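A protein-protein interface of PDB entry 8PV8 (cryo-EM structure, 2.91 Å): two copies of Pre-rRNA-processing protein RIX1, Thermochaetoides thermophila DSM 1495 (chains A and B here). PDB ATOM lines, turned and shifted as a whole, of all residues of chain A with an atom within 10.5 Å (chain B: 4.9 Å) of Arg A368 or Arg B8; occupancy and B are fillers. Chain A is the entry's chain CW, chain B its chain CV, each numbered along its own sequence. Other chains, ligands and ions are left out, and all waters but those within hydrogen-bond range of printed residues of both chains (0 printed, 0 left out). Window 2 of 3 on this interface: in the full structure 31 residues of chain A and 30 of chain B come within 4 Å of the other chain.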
ATOM      1  N   ARG A 267      -6.615  -5.919   2.659  1.00  0.00           N
ATOM      2  CA  ARG A 267      -6.974  -7.317   2.426  1.00  0.00           C
ATOM      3  C   ARG A 267      -6.438  -7.841   1.095  1.00  0.00           C
ATOM      4  O   ARG A 267      -6.312  -9.057   0.909  1.00  0.00           O
ATOM      5  CB  ARG A 267      -8.492  -7.475   2.506  1.00  0.00           C
ATOM      6  CG  ARG A 267      -9.272  -6.601   1.545  1.00  0.00           C
ATOM      7  CD  ARG A 267     -10.759  -6.667   1.855  1.00  0.00           C
ATOM      8  NE  ARG A 267     -11.411  -7.838   1.287  1.00  0.00           N
ATOM      9  CZ  ARG A 267     -12.072  -7.820   0.139  1.00  0.00           C
ATOM     10  NH1 ARG A 267     -12.234  -6.701  -0.545  1.00  0.00           N
ATOM     11  NH2 ARG A 267     -12.598  -8.950  -0.326  1.00  0.00           N
ATOM     12  N   ALA A 268      -6.119  -6.948   0.155  1.00  0.00           N
ATOM     13  CA  ALA A 268      -5.540  -7.388  -1.111  1.00  0.00           C
ATOM     14  C   ALA A 268      -4.105  -7.881  -0.936  1.00  0.00           C
ATOM     15  O   ALA A 268      -3.675  -8.815  -1.622  1.00  0.00           O
ATOM     16  CB  ALA A 268      -5.596  -6.258  -2.138  1.00  0.00           C
ATOM     17  N   ALA A 286     -13.372 -12.679   1.767  1.00  0.00           N
ATOM     18  CA  ALA A 286     -12.800 -12.408   0.453  1.00  0.00           C
ATOM     19  C   ALA A 286     -13.844 -11.850  -0.506  1.00  0.00           C
ATOM     20  O   ALA A 286     -13.524 -11.025  -1.370  1.00  0.00           O
ATOM     21  CB  ALA A 286     -12.172 -13.680  -0.117  1.00  0.00           C
ATOM     22  N   LEU A 306     -13.411   0.576  -1.133  1.00  0.00           N
ATOM     23  CA  LEU A 306     -12.016   0.655  -0.718  1.00  0.00           C
ATOM     24  C   LEU A 306     -11.545   2.099  -0.605  1.00  0.00           C
ATOM     25  O   LEU A 306     -10.721   2.422   0.260  1.00  0.00           O
ATOM     26  CB  LEU A 306     -11.141  -0.122  -1.694  1.00  0.00           C
ATOM     27  CG  LEU A 306      -9.744  -0.450  -1.183  1.00  0.00           C
ATOM     28  CD1 LEU A 306      -9.798  -1.562  -0.157  1.00  0.00           C
ATOM     29  CD2 LEU A 306      -8.897  -0.858  -2.350  1.00  0.00           C
ATOM     30  N   PRO A 352       4.135  -0.230  -5.819  1.00  0.00           N
ATOM     31  CA  PRO A 352       5.266  -0.779  -6.575  1.00  0.00           C
ATOM     32  C   PRO A 352       5.899   0.287  -7.452  1.00  0.00           C
ATOM     33  O   PRO A 352       5.334   1.365  -7.657  1.00  0.00           O
ATOM     34  CB  PRO A 352       4.617  -1.867  -7.434  1.00  0.00           C
ATOM     35  CG  PRO A 352       3.404  -2.244  -6.723  1.00  0.00           C
ATOM     36  CD  PRO A 352       2.900  -0.980  -6.097  1.00  0.00           C
ATOM     37  N   LEU A 354       7.184   0.521 -11.569  1.00  0.00           N
ATOM     38  CA  LEU A 354       6.535   0.011 -12.769  1.00  0.00           C
ATOM     39  C   LEU A 354       7.033  -1.396 -13.085  1.00  0.00           C
ATOM     40  O   LEU A 354       8.147  -1.586 -13.578  1.00  0.00           O
ATOM     41  CB  LEU A 354       6.777   0.955 -13.947  1.00  0.00           C
ATOM     42  CG  LEU A 354       5.836   0.777 -15.144  1.00  0.00           C
ATOM     43  CD1 LEU A 354       4.381   0.794 -14.698  1.00  0.00           C
ATOM     44  CD2 LEU A 354       6.078   1.854 -16.193  1.00  0.00           C
ATOM     45  N   GLY A 355       6.193  -2.389 -12.786  1.00  0.00           N
ATOM     46  CA  GLY A 355       6.524  -3.780 -13.023  1.00  0.00           C
ATOM     47  C   GLY A 355       6.793  -4.621 -11.791  1.00  0.00           C
ATOM     48  O   GLY A 355       7.236  -5.768 -11.935  1.00  0.00           O
ATOM     49  N   GLU A 357       4.350  -5.322  -9.550  1.00  0.00           N
ATOM     50  CA  GLU A 357       3.073  -5.883  -9.121  1.00  0.00           C
ATOM     51  C   GLU A 357       3.140  -7.400  -9.021  1.00  0.00           C
ATOM     52  O   GLU A 357       2.583  -7.997  -8.092  1.00  0.00           O
ATOM     53  CB  GLU A 357       1.969  -5.454 -10.088  1.00  0.00           C
ATOM     54  CG  GLU A 357       0.557  -5.601  -9.548  1.00  0.00           C
ATOM     55  CD  GLU A 357      -0.091  -6.909  -9.958  1.00  0.00           C
ATOM     56  OE1 GLU A 357       0.254  -7.432 -11.039  1.00  0.00           O
ATOM     57  OE2 GLU A 357      -0.947  -7.412  -9.202  1.00  0.00           O
ATOM     58  N   ASP A 358       3.820  -8.045  -9.972  1.00  0.00           N
ATOM     59  CA  ASP A 358       4.022  -9.486  -9.880  1.00  0.00           C
ATOM     60  C   ASP A 358       5.025  -9.829  -8.786  1.00  0.00           C
ATOM     61  O   ASP A 358       4.997 -10.935  -8.232  1.00  0.00           O
ATOM     62  CB  ASP A 358       4.489 -10.038 -11.227  1.00  0.00           C
ATOM     63  CG  ASP A 358       3.545  -9.688 -12.359  1.00  0.00           C
ATOM     64  OD1 ASP A 358       2.480  -9.097 -12.084  1.00  0.00           O
ATOM     65  OD2 ASP A 358       3.866 -10.008 -13.522  1.00  0.00           O
ATOM     66  N   THR A 362       0.165 -10.724  -3.455  1.00  0.00           N
ATOM     67  CA  THR A 362      -1.200 -10.215  -3.480  1.00  0.00           C
ATOM     68  C   THR A 362      -2.185 -11.357  -3.286  1.00  0.00           C
ATOM     69  O   THR A 362      -1.863 -12.524  -3.525  1.00  0.00           O
ATOM     70  CB  THR A 362      -1.526  -9.501  -4.802  1.00  0.00           C
ATOM     71  OG1 THR A 362      -1.182 -10.350  -5.904  1.00  0.00           O
ATOM     72  CG2 THR A 362      -0.768  -8.195  -4.916  1.00  0.00           C
ATOM     73  N   ASN A 363      -3.391 -11.006  -2.843  1.00  0.00           N
ATOM     74  CA  ASN A 363      -4.468 -11.981  -2.763  1.00  0.00           C
ATOM     75  C   ASN A 363      -4.901 -12.387  -4.170  1.00  0.00           C
ATOM     76  O   ASN A 363      -5.061 -11.528  -5.043  1.00  0.00           O
ATOM     77  CB  ASN A 363      -5.657 -11.408  -1.989  1.00  0.00           C
ATOM     78  CG  ASN A 363      -6.765 -12.426  -1.761  1.00  0.00           C
ATOM     79  OD1 ASN A 363      -7.512 -12.769  -2.677  1.00  0.00           O
ATOM     80  ND2 ASN A 363      -6.874 -12.913  -0.532  1.00  0.00           N
ATOM     81  N   PRO A 364      -5.094 -13.684  -4.423  1.00  0.00           N
ATOM     82  CA  PRO A 364      -5.513 -14.100  -5.773  1.00  0.00           C
ATOM     83  C   PRO A 364      -6.982 -13.842  -6.059  1.00  0.00           C
ATOM     84  O   PRO A 364      -7.343 -13.558  -7.209  1.00  0.00           O
ATOM     85  CB  PRO A 364      -5.189 -15.601  -5.786  1.00  0.00           C
ATOM     86  CG  PRO A 364      -5.244 -16.007  -4.345  1.00  0.00           C
ATOM     87  CD  PRO A 364      -4.720 -14.830  -3.576  1.00  0.00           C
ATOM     88  N   ALA A 365      -7.846 -13.941  -5.047  1.00  0.00           N
ATOM     89  CA  ALA A 365      -9.284 -13.862  -5.291  1.00  0.00           C
ATOM     90  C   ALA A 365      -9.743 -12.425  -5.507  1.00  0.00           C
ATOM     91  O   ALA A 365     -10.762 -12.185  -6.167  1.00  0.00           O
ATOM     92  CB  ALA A 365     -10.046 -14.499  -4.131  1.00  0.00           C
ATOM     93  N   ILE A 366      -9.013 -11.456  -4.948  1.00  0.00           N
ATOM     94  CA  ILE A 366      -9.487 -10.077  -4.950  1.00  0.00           C
ATOM     95  C   ILE A 366      -9.345  -9.488  -6.350  1.00  0.00           C
ATOM     96  O   ILE A 366      -8.503  -9.923  -7.148  1.00  0.00           O
ATOM     97  CB  ILE A 366      -8.732  -9.265  -3.881  1.00  0.00           C
ATOM     98  CG1 ILE A 366      -9.407  -7.919  -3.624  1.00  0.00           C
ATOM     99  CG2 ILE A 366      -7.292  -9.040  -4.285  1.00  0.00           C
ATOM    100  CD1 ILE A 366     -10.834  -8.065  -3.208  1.00  0.00           C
ATOM    101  N   GLY A 367     -10.206  -8.512  -6.673  1.00  0.00           N
ATOM    102  CA  GLY A 367     -10.236  -7.931  -7.997  1.00  0.00           C
ATOM    103  C   GLY A 367      -9.032  -7.055  -8.326  1.00  0.00           C
ATOM    104  O   GLY A 367      -8.438  -6.392  -7.475  1.00  0.00           O
ATOM    105  N   ARG A 368      -8.694  -7.049  -9.616  1.00  0.00           N
ATOM    106  CA  ARG A 368      -7.586  -6.239 -10.111  1.00  0.00           C
ATOM    107  C   ARG A 368      -7.936  -4.752 -10.118  1.00  0.00           C
ATOM    108  O   ARG A 368      -7.063  -3.900  -9.900  1.00  0.00           O
ATOM    109  CB  ARG A 368      -7.173  -6.783 -11.487  1.00  0.00           C
ATOM    110  CG  ARG A 368      -5.924  -6.212 -12.155  1.00  0.00           C
ATOM    111  CD  ARG A 368      -6.291  -5.039 -13.048  1.00  0.00           C
ATOM    112  NE  ARG A 368      -7.191  -5.524 -14.091  1.00  0.00           N
ATOM    113  CZ  ARG A 368      -7.957  -4.762 -14.860  1.00  0.00           C
ATOM    114  NH1 ARG A 368      -8.003  -3.452 -14.707  1.00  0.00           N
ATOM    115  NH2 ARG A 368      -8.701  -5.332 -15.802  1.00  0.00           N
ATOM    116  N   ASP A 369      -9.211  -4.419 -10.342  1.00  0.00           N
ATOM    117  CA  ASP A 369      -9.657  -3.034 -10.206  1.00  0.00           C
ATOM    118  C   ASP A 369      -9.520  -2.550  -8.765  1.00  0.00           C
ATOM    119  O   ASP A 369      -9.069  -1.424  -8.514  1.00  0.00           O
ATOM    120  CB  ASP A 369     -11.104  -2.902 -10.680  1.00  0.00           C
ATOM    121  CG  ASP A 369     -11.263  -3.160 -12.166  1.00  0.00           C
ATOM    122  OD1 ASP A 369     -10.324  -2.862 -12.935  1.00  0.00           O
ATOM    123  OD2 ASP A 369     -12.334  -3.664 -12.562  1.00  0.00           O
ATOM    124  N   GLU A 370      -9.909  -3.394  -7.804  1.00  0.00           N
ATOM    125  CA  GLU A 370      -9.740  -3.059  -6.393  1.00  0.00           C
ATOM    126  C   GLU A 370      -8.264  -2.945  -6.034  1.00  0.00           C
ATOM    127  O   GLU A 370      -7.877  -2.103  -5.216  1.00  0.00           O
ATOM    128  CB  GLU A 370     -10.440  -4.106  -5.521  1.00  0.00           C
ATOM    129  CG  GLU A 370     -10.294  -3.889  -4.021  1.00  0.00           C
ATOM    130  CD  GLU A 370     -11.376  -4.590  -3.223  1.00  0.00           C
ATOM    131  OE1 GLU A 370     -12.394  -4.991  -3.824  1.00  0.00           O
ATOM    132  OE2 GLU A 370     -11.210  -4.738  -1.993  1.00  0.00           O
ATOM    133  N   LYS A 371      -7.423  -3.783  -6.647  1.00  0.00           N
ATOM    134  CA  LYS A 371      -5.980  -3.675  -6.452  1.00  0.00           C
ATOM    135  C   LYS A 371      -5.452  -2.321  -6.917  1.00  0.00           C
ATOM    136  O   LYS A 371      -4.698  -1.652  -6.197  1.00  0.00           O
ATOM    137  CB  LYS A 371      -5.273  -4.805  -7.198  1.00  0.00           C
ATOM    138  CG  LYS A 371      -5.323  -6.163  -6.530  1.00  0.00           C
ATOM    139  CD  LYS A 371      -4.578  -7.179  -7.379  1.00  0.00           C
ATOM    140  CE  LYS A 371      -4.634  -8.568  -6.779  1.00  0.00           C
ATOM    141  NZ  LYS A 371      -4.046  -9.576  -7.699  1.00  0.00           N
ATOM    142  N   ALA A 372      -5.852  -1.901  -8.122  1.00  0.00           N
ATOM    143  CA  ALA A 372      -5.409  -0.613  -8.651  1.00  0.00           C
ATOM    144  C   ALA A 372      -5.903   0.537  -7.781  1.00  0.00           C
ATOM    145  O   ALA A 372      -5.168   1.505  -7.541  1.00  0.00           O
ATOM    146  CB  ALA A 372      -5.890  -0.446 -10.090  1.00  0.00           C
ATOM    147  N   GLU A 373      -7.137   0.427  -7.279  1.00  0.00           N
ATOM    148  CA  GLU A 373      -7.657   1.399  -6.322  1.00  0.00           C
ATOM    149  C   GLU A 373      -6.819   1.440  -5.048  1.00  0.00           C
ATOM    150  O   GLU A 373      -6.554   2.525  -4.514  1.00  0.00           O
ATOM    151  CB  GLU A 373      -9.111   1.061  -5.995  1.00  0.00           C
ATOM    152  CG  GLU A 373      -9.881   2.150  -5.275  1.00  0.00           C
ATOM    153  CD  GLU A 373     -11.377   1.904  -5.307  1.00  0.00           C
ATOM    154  OE1 GLU A 373     -11.825   1.084  -6.136  1.00  0.00           O
ATOM    155  OE2 GLU A 373     -12.104   2.522  -4.502  1.00  0.00           O
ATOM    156  N   LEU A 374      -6.374   0.275  -4.567  1.00  0.00           N
ATOM    157  CA  LEU A 374      -5.534   0.226  -3.373  1.00  0.00           C
ATOM    158  C   LEU A 374      -4.200   0.925  -3.589  1.00  0.00           C
ATOM    159  O   LEU A 374      -3.767   1.718  -2.738  1.00  0.00           O
ATOM    160  CB  LEU A 374      -5.299  -1.222  -2.949  1.00  0.00           C
ATOM    161  CG  LEU A 374      -4.426  -1.391  -1.705  1.00  0.00           C
ATOM    162  CD1 LEU A 374      -4.964  -0.580  -0.538  1.00  0.00           C
ATOM    163  CD2 LEU A 374      -4.313  -2.853  -1.327  1.00  0.00           C
ATOM    164  N   TRP A 375      -3.520   0.642  -4.703  1.00  0.00           N
ATOM    165  CA  TRP A 375      -2.212   1.276  -4.779  1.00  0.00           C
ATOM    166  C   TRP A 375      -2.305   2.704  -5.298  1.00  0.00           C
ATOM    167  O   TRP A 375      -1.300   3.420  -5.264  1.00  0.00           O
ATOM    168  CB  TRP A 375      -1.171   0.520  -5.612  1.00  0.00           C
ATOM    169  CG  TRP A 375      -0.733  -0.770  -4.986  1.00  0.00           C
ATOM    170  CD1 TRP A 375       0.268  -0.935  -4.087  1.00  0.00           C
ATOM    171  CD2 TRP A 375      -1.026  -2.085  -5.472  1.00  0.00           C
ATOM    172  NE1 TRP A 375       0.473  -2.264  -3.827  1.00  0.00           N
ATOM    173  CE2 TRP A 375      -0.294  -2.994  -4.691  1.00  0.00           C
ATOM    174  CE3 TRP A 375      -1.881  -2.584  -6.451  1.00  0.00           C
ATOM    175  CZ2 TRP A 375      -0.408  -4.370  -4.848  1.00  0.00           C
ATOM    176  CZ3 TRP A 375      -1.996  -3.941  -6.599  1.00  0.00           C
ATOM    177  CH2 TRP A 375      -1.265  -4.820  -5.808  1.00  0.00           C
ATOM    178  N   SER A 376      -3.473   3.135  -5.774  1.00  0.00           N
ATOM    179  CA  SER A 376      -3.721   4.560  -5.930  1.00  0.00           C
ATOM    180  C   SER A 376      -4.037   5.245  -4.609  1.00  0.00           C
ATOM    181  O   SER A 376      -3.771   6.441  -4.464  1.00  0.00           O
ATOM    182  CB  SER A 376      -4.874   4.804  -6.911  1.00  0.00           C
ATOM    183  OG  SER A 376      -6.110   4.371  -6.374  1.00  0.00           O
ATOM    184  N   THR B   2       1.204  -1.474 -18.838  1.00  0.00           N
ATOM    185  CA  THR B   2      -0.229  -1.237 -18.956  1.00  0.00           C
ATOM    186  C   THR B   2      -0.587   0.183 -18.532  1.00  0.00           C
ATOM    187  O   THR B   2       0.281   1.050 -18.435  1.00  0.00           O
ATOM    188  CB  THR B   2      -1.041  -2.233 -18.109  1.00  0.00           C
ATOM    189  OG1 THR B   2      -0.739  -2.043 -16.722  1.00  0.00           O
ATOM    190  CG2 THR B   2      -0.710  -3.663 -18.505  1.00  0.00           C
ATOM    191  N   ALA B   3      -1.874   0.410 -18.287  1.00  0.00           N
ATOM    192  CA  ALA B   3      -2.332   1.727 -17.878  1.00  0.00           C
ATOM    193  C   ALA B   3      -1.904   2.015 -16.440  1.00  0.00           C
ATOM    194  O   ALA B   3      -1.768   1.088 -15.636  1.00  0.00           O
ATOM    195  CB  ALA B   3      -3.850   1.828 -18.000  1.00  0.00           C
ATOM    196  N   PRO B   4      -1.654   3.279 -16.099  1.00  0.00           N
ATOM    197  CA  PRO B   4      -1.389   3.614 -14.705  1.00  0.00           C
ATOM    198  C   PRO B   4      -2.618   3.379 -13.853  1.00  0.00           C
ATOM    199  O   PRO B   4      -3.764   3.525 -14.324  1.00  0.00           O
ATOM    200  CB  PRO B   4      -1.020   5.103 -14.766  1.00  0.00           C
ATOM    201  CG  PRO B   4      -0.518   5.310 -16.143  1.00  0.00           C
ATOM    202  CD  PRO B   4      -1.331   4.391 -17.007  1.00  0.00           C
ATOM    203  N   PRO B   5      -2.429   2.989 -12.586  1.00  0.00           N
ATOM    204  CA  PRO B   5      -3.583   2.783 -11.695  1.00  0.00           C
ATOM    205  C   PRO B   5      -4.417   4.032 -11.470  1.00  0.00           C
ATOM    206  O   PRO B   5      -5.638   3.924 -11.327  1.00  0.00           O
ATOM    207  CB  PRO B   5      -2.933   2.288 -10.393  1.00  0.00           C
ATOM    208  CG  PRO B   5      -1.508   2.719 -10.476  1.00  0.00           C
ATOM    209  CD  PRO B   5      -1.152   2.674 -11.925  1.00  0.00           C
ATOM    210  N   ASP B   6      -3.795   5.213 -11.451  1.00  0.00           N
ATOM    211  CA  ASP B   6      -4.548   6.453 -11.280  1.00  0.00           C
ATOM    212  C   ASP B   6      -5.495   6.686 -12.451  1.00  0.00           C
ATOM    213  O   ASP B   6      -6.669   7.024 -12.257  1.00  0.00           O
ATOM    214  CB  ASP B   6      -3.582   7.627 -11.123  1.00  0.00           C
ATOM    215  CG  ASP B   6      -2.587   7.413 -10.001  1.00  0.00           C
ATOM    216  OD1 ASP B   6      -3.013   7.041  -8.887  1.00  0.00           O
ATOM    217  OD2 ASP B   6      -1.377   7.608 -10.236  1.00  0.00           O
ATOM    218  N   LEU B   7      -5.004   6.482 -13.677  1.00  0.00           N
ATOM    219  CA  LEU B   7      -5.849   6.617 -14.861  1.00  0.00           C
ATOM    220  C   LEU B   7      -6.945   5.560 -14.879  1.00  0.00           C
ATOM    221  O   LEU B   7      -8.081   5.837 -15.291  1.00  0.00           O
ATOM    222  CB  LEU B   7      -4.994   6.521 -16.124  1.00  0.00           C
ATOM    223  CG  LEU B   7      -5.692   6.601 -17.480  1.00  0.00           C
ATOM    224  CD1 LEU B   7      -6.513   7.877 -17.590  1.00  0.00           C
ATOM    225  CD2 LEU B   7      -4.664   6.525 -18.596  1.00  0.00           C
ATOM    226  N   ARG B   8      -6.620   4.345 -14.432  1.00  0.00           N
ATOM    227  CA  ARG B   8      -7.617   3.280 -14.360  1.00  0.00           C
ATOM    228  C   ARG B   8      -8.746   3.637 -13.398  1.00  0.00           C
ATOM    229  O   ARG B   8      -9.931   3.478 -13.725  1.00  0.00           O
ATOM    230  CB  ARG B   8      -6.937   1.979 -13.943  1.00  0.00           C
ATOM    231  CG  ARG B   8      -7.772   0.740 -14.146  1.00  0.00           C
ATOM    232  CD  ARG B   8      -6.961  -0.505 -13.850  1.00  0.00           C
ATOM    233  NE  ARG B   8      -5.826  -0.670 -14.751  1.00  0.00           N
ATOM    234  CZ  ARG B   8      -4.556  -0.552 -14.390  1.00  0.00           C
ATOM    235  NH1 ARG B   8      -4.216  -0.274 -13.143  1.00  0.00           N
ATOM    236  NH2 ARG B   8      -3.603  -0.722 -15.303  1.00  0.00           N
ATOM    237  N   VAL B   9      -8.395   4.143 -12.211  1.00  0.00           N
ATOM    238  CA  VAL B   9      -9.405   4.545 -11.233  1.00  0.00           C
ATOM    239  C   VAL B   9     -10.212   5.731 -11.747  1.00  0.00           C
ATOM    240  O   VAL B   9     -11.427   5.799 -11.533  1.00  0.00           O
ATOM    241  CB  VAL B   9      -8.752   4.835  -9.867  1.00  0.00           C
ATOM    242  CG1 VAL B   9      -9.788   5.282  -8.848  1.00  0.00           C
ATOM    243  CG2 VAL B   9      -8.089   3.585  -9.337  1.00  0.00           C
ATOM    244  N   VAL B  10      -9.563   6.667 -12.451  1.00  0.00           N
ATOM    245  CA  VAL B  10     -10.284   7.807 -13.022  1.00  0.00           C
ATOM    246  C   VAL B  10     -11.340   7.332 -14.012  1.00  0.00           C
ATOM    247  O   VAL B  10     -12.511   7.731 -13.937  1.00  0.00           O
ATOM    248  CB  VAL B  10      -9.307   8.796 -13.684  1.00  0.00           C
ATOM    249  CG1 VAL B  10     -10.053   9.743 -14.591  1.00  0.00           C
ATOM    250  CG2 VAL B  10      -8.602   9.603 -12.643  1.00  0.00           C
ATOM    251  N   CYS B  11     -10.949   6.439 -14.928  1.00  0.00           N
ATOM    252  CA  CYS B  11     -11.895   5.931 -15.919  1.00  0.00           C
ATOM    253  C   CYS B  11     -13.015   5.127 -15.266  1.00  0.00           C
ATOM    254  O   CYS B  11     -14.179   5.237 -15.668  1.00  0.00           O
ATOM    255  CB  CYS B  11     -11.162   5.088 -16.962  1.00  0.00           C
ATOM    256  SG  CYS B  11      -9.936   6.002 -17.923  1.00  0.00           S
ATOM    257  N   HIS B  12     -12.691   4.340 -14.238  1.00  0.00           N
ATOM    258  CA  HIS B  12     -13.702   3.482 -13.624  1.00  0.00           C
ATOM    259  C   HIS B  12     -14.701   4.297 -12.803  1.00  0.00           C
ATOM    260  O   HIS B  12     -15.909   4.035 -12.843  1.00  0.00           O
ATOM    261  CB  HIS B  12     -13.016   2.414 -12.772  1.00  0.00           C
ATOM    262  CG  HIS B  12     -13.964   1.449 -12.133  1.00  0.00           C
ATOM    263  ND1 HIS B  12     -14.609   0.460 -12.844  1.00  0.00           N
ATOM    264  CD2 HIS B  12     -14.359   1.305 -10.847  1.00  0.00           C
ATOM    265  CE1 HIS B  12     -15.371  -0.243 -12.025  1.00  0.00           C
ATOM    266  NE2 HIS B  12     -15.238   0.251 -10.808  1.00  0.00           N
ATOM    267  N   GLU B  54      -3.448   0.272 -23.974  1.00  0.00           N
ATOM    268  CA  GLU B  54      -4.485   0.531 -22.981  1.00  0.00           C
ATOM    269  C   GLU B  54      -4.392   1.956 -22.450  1.00  0.00           C
ATOM    270  O   GLU B  54      -5.417   2.583 -22.154  1.00  0.00           O
ATOM    271  CB  GLU B  54      -4.373  -0.481 -21.839  1.00  0.00           C
ATOM    272  CG  GLU B  54      -5.415  -0.325 -20.739  1.00  0.00           C
ATOM    273  CD  GLU B  54      -5.148  -1.224 -19.546  1.00  0.00           C
ATOM    274  OE1 GLU B  54      -4.173  -2.003 -19.594  1.00  0.00           O
ATOM    275  OE2 GLU B  54      -5.912  -1.150 -18.561  1.00  0.00           O
ATOM    276  N   LEU B  58      -7.475   4.551 -22.730  1.00  0.00           N
ATOM    277  CA  LEU B  58      -8.051   5.187 -21.552  1.00  0.00           C
ATOM    278  C   LEU B  58      -7.956   6.706 -21.630  1.00  0.00           C
ATOM    279  O   LEU B  58      -8.868   7.406 -21.183  1.00  0.00           O
ATOM    280  CB  LEU B  58      -7.383   4.663 -20.281  1.00  0.00           C
ATOM    281  CG  LEU B  58      -7.745   3.238 -19.853  1.00  0.00           C
ATOM    282  CD1 LEU B  58      -7.339   2.996 -18.409  1.00  0.00           C
ATOM    283  CD2 LEU B  58      -9.230   2.959 -20.043  1.00  0.00           C
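OE2 of Glu B54 is in salt-bridge range of NE of Arg B8, at 3.8 Å. NH2 of Arg B8 is in hydrogen-bond range of OG1 of Thr B2, at 3.5 Å. The guanidinium group (NH2) of Arg B8 sits at hydrogen-bond distance from the backbone carbonyl oxygen (O) of Ala B3 (2.6 Å). OD1 of Asp A369 lies within salt-bridge range of NH1 of Arg A368, at 3.0 Å. O of Glu A373 sits at hydrogen-bond distance from OG of Ser A376 (2.7 Å). The backbone carbonyl oxygen (O) of Ala A372 is in hydrogen-bond range of the side-chain hydroxyl (OG) of Ser A376 (3.2 Å).
Arg B8 touches Arg A368. Ala A372 touches Pro B5. Ala A372 touches Arg B8. Glu A373 touches Val B9. Asp B6 touches Ser A376. Ser A376 touches Val B9 (OG to CG2, 3.6 Å).
Arg A368 touches one residue of chain B. Of the printed residues of chain A, Arg B8 touches Arg A368 (3.2 Å) and Ala A372 (3.5 Å). No residue of chain A comes within 4 Å of Thr B2. Ala B3 touches none of the printed residues of chain A. Pro B4 touches none of the printed residues of chain A. Pro B5 touches just one residue of chain A: Ala A372 (3.7 Å). No residue of chain A comes within 4 Å of Leu B7. No residue of chain A comes within 4 Å of Cys B11. Of the printed residues of chain A, Asp B6 touches Ser A376 (3.5 Å). Of the printed residues of chain B, Ala A372 touches Pro B5 and Arg B8. Of the printed residues of chain B, Ser A376 touches Asp B6 (3.5 Å) and Val B9 (3.6 Å). The nearest printed residue of chain B that does not touch Arg A368 is Glu B54 (5.0 Å). The nearest residue of chain A that does not touch Arg B8 is Asp A369 (4.2 Å). The nearest printed residue of chain A that does not touch Asp B6 is Trp A375 (5.4 Å).
Of the 24 printed residues of chain A, 4 touch a printed residue of chain B. Hydrophobic or aromatic side chains of chain A that line the printed part of chain B: Ala A372. Among the printed residues, 6 pairs touch across the chains.
No position is printed for both chains. Of the 6 pairs that touch across the chains among the printed residues, none has its exchanged pair printed and touching as well.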
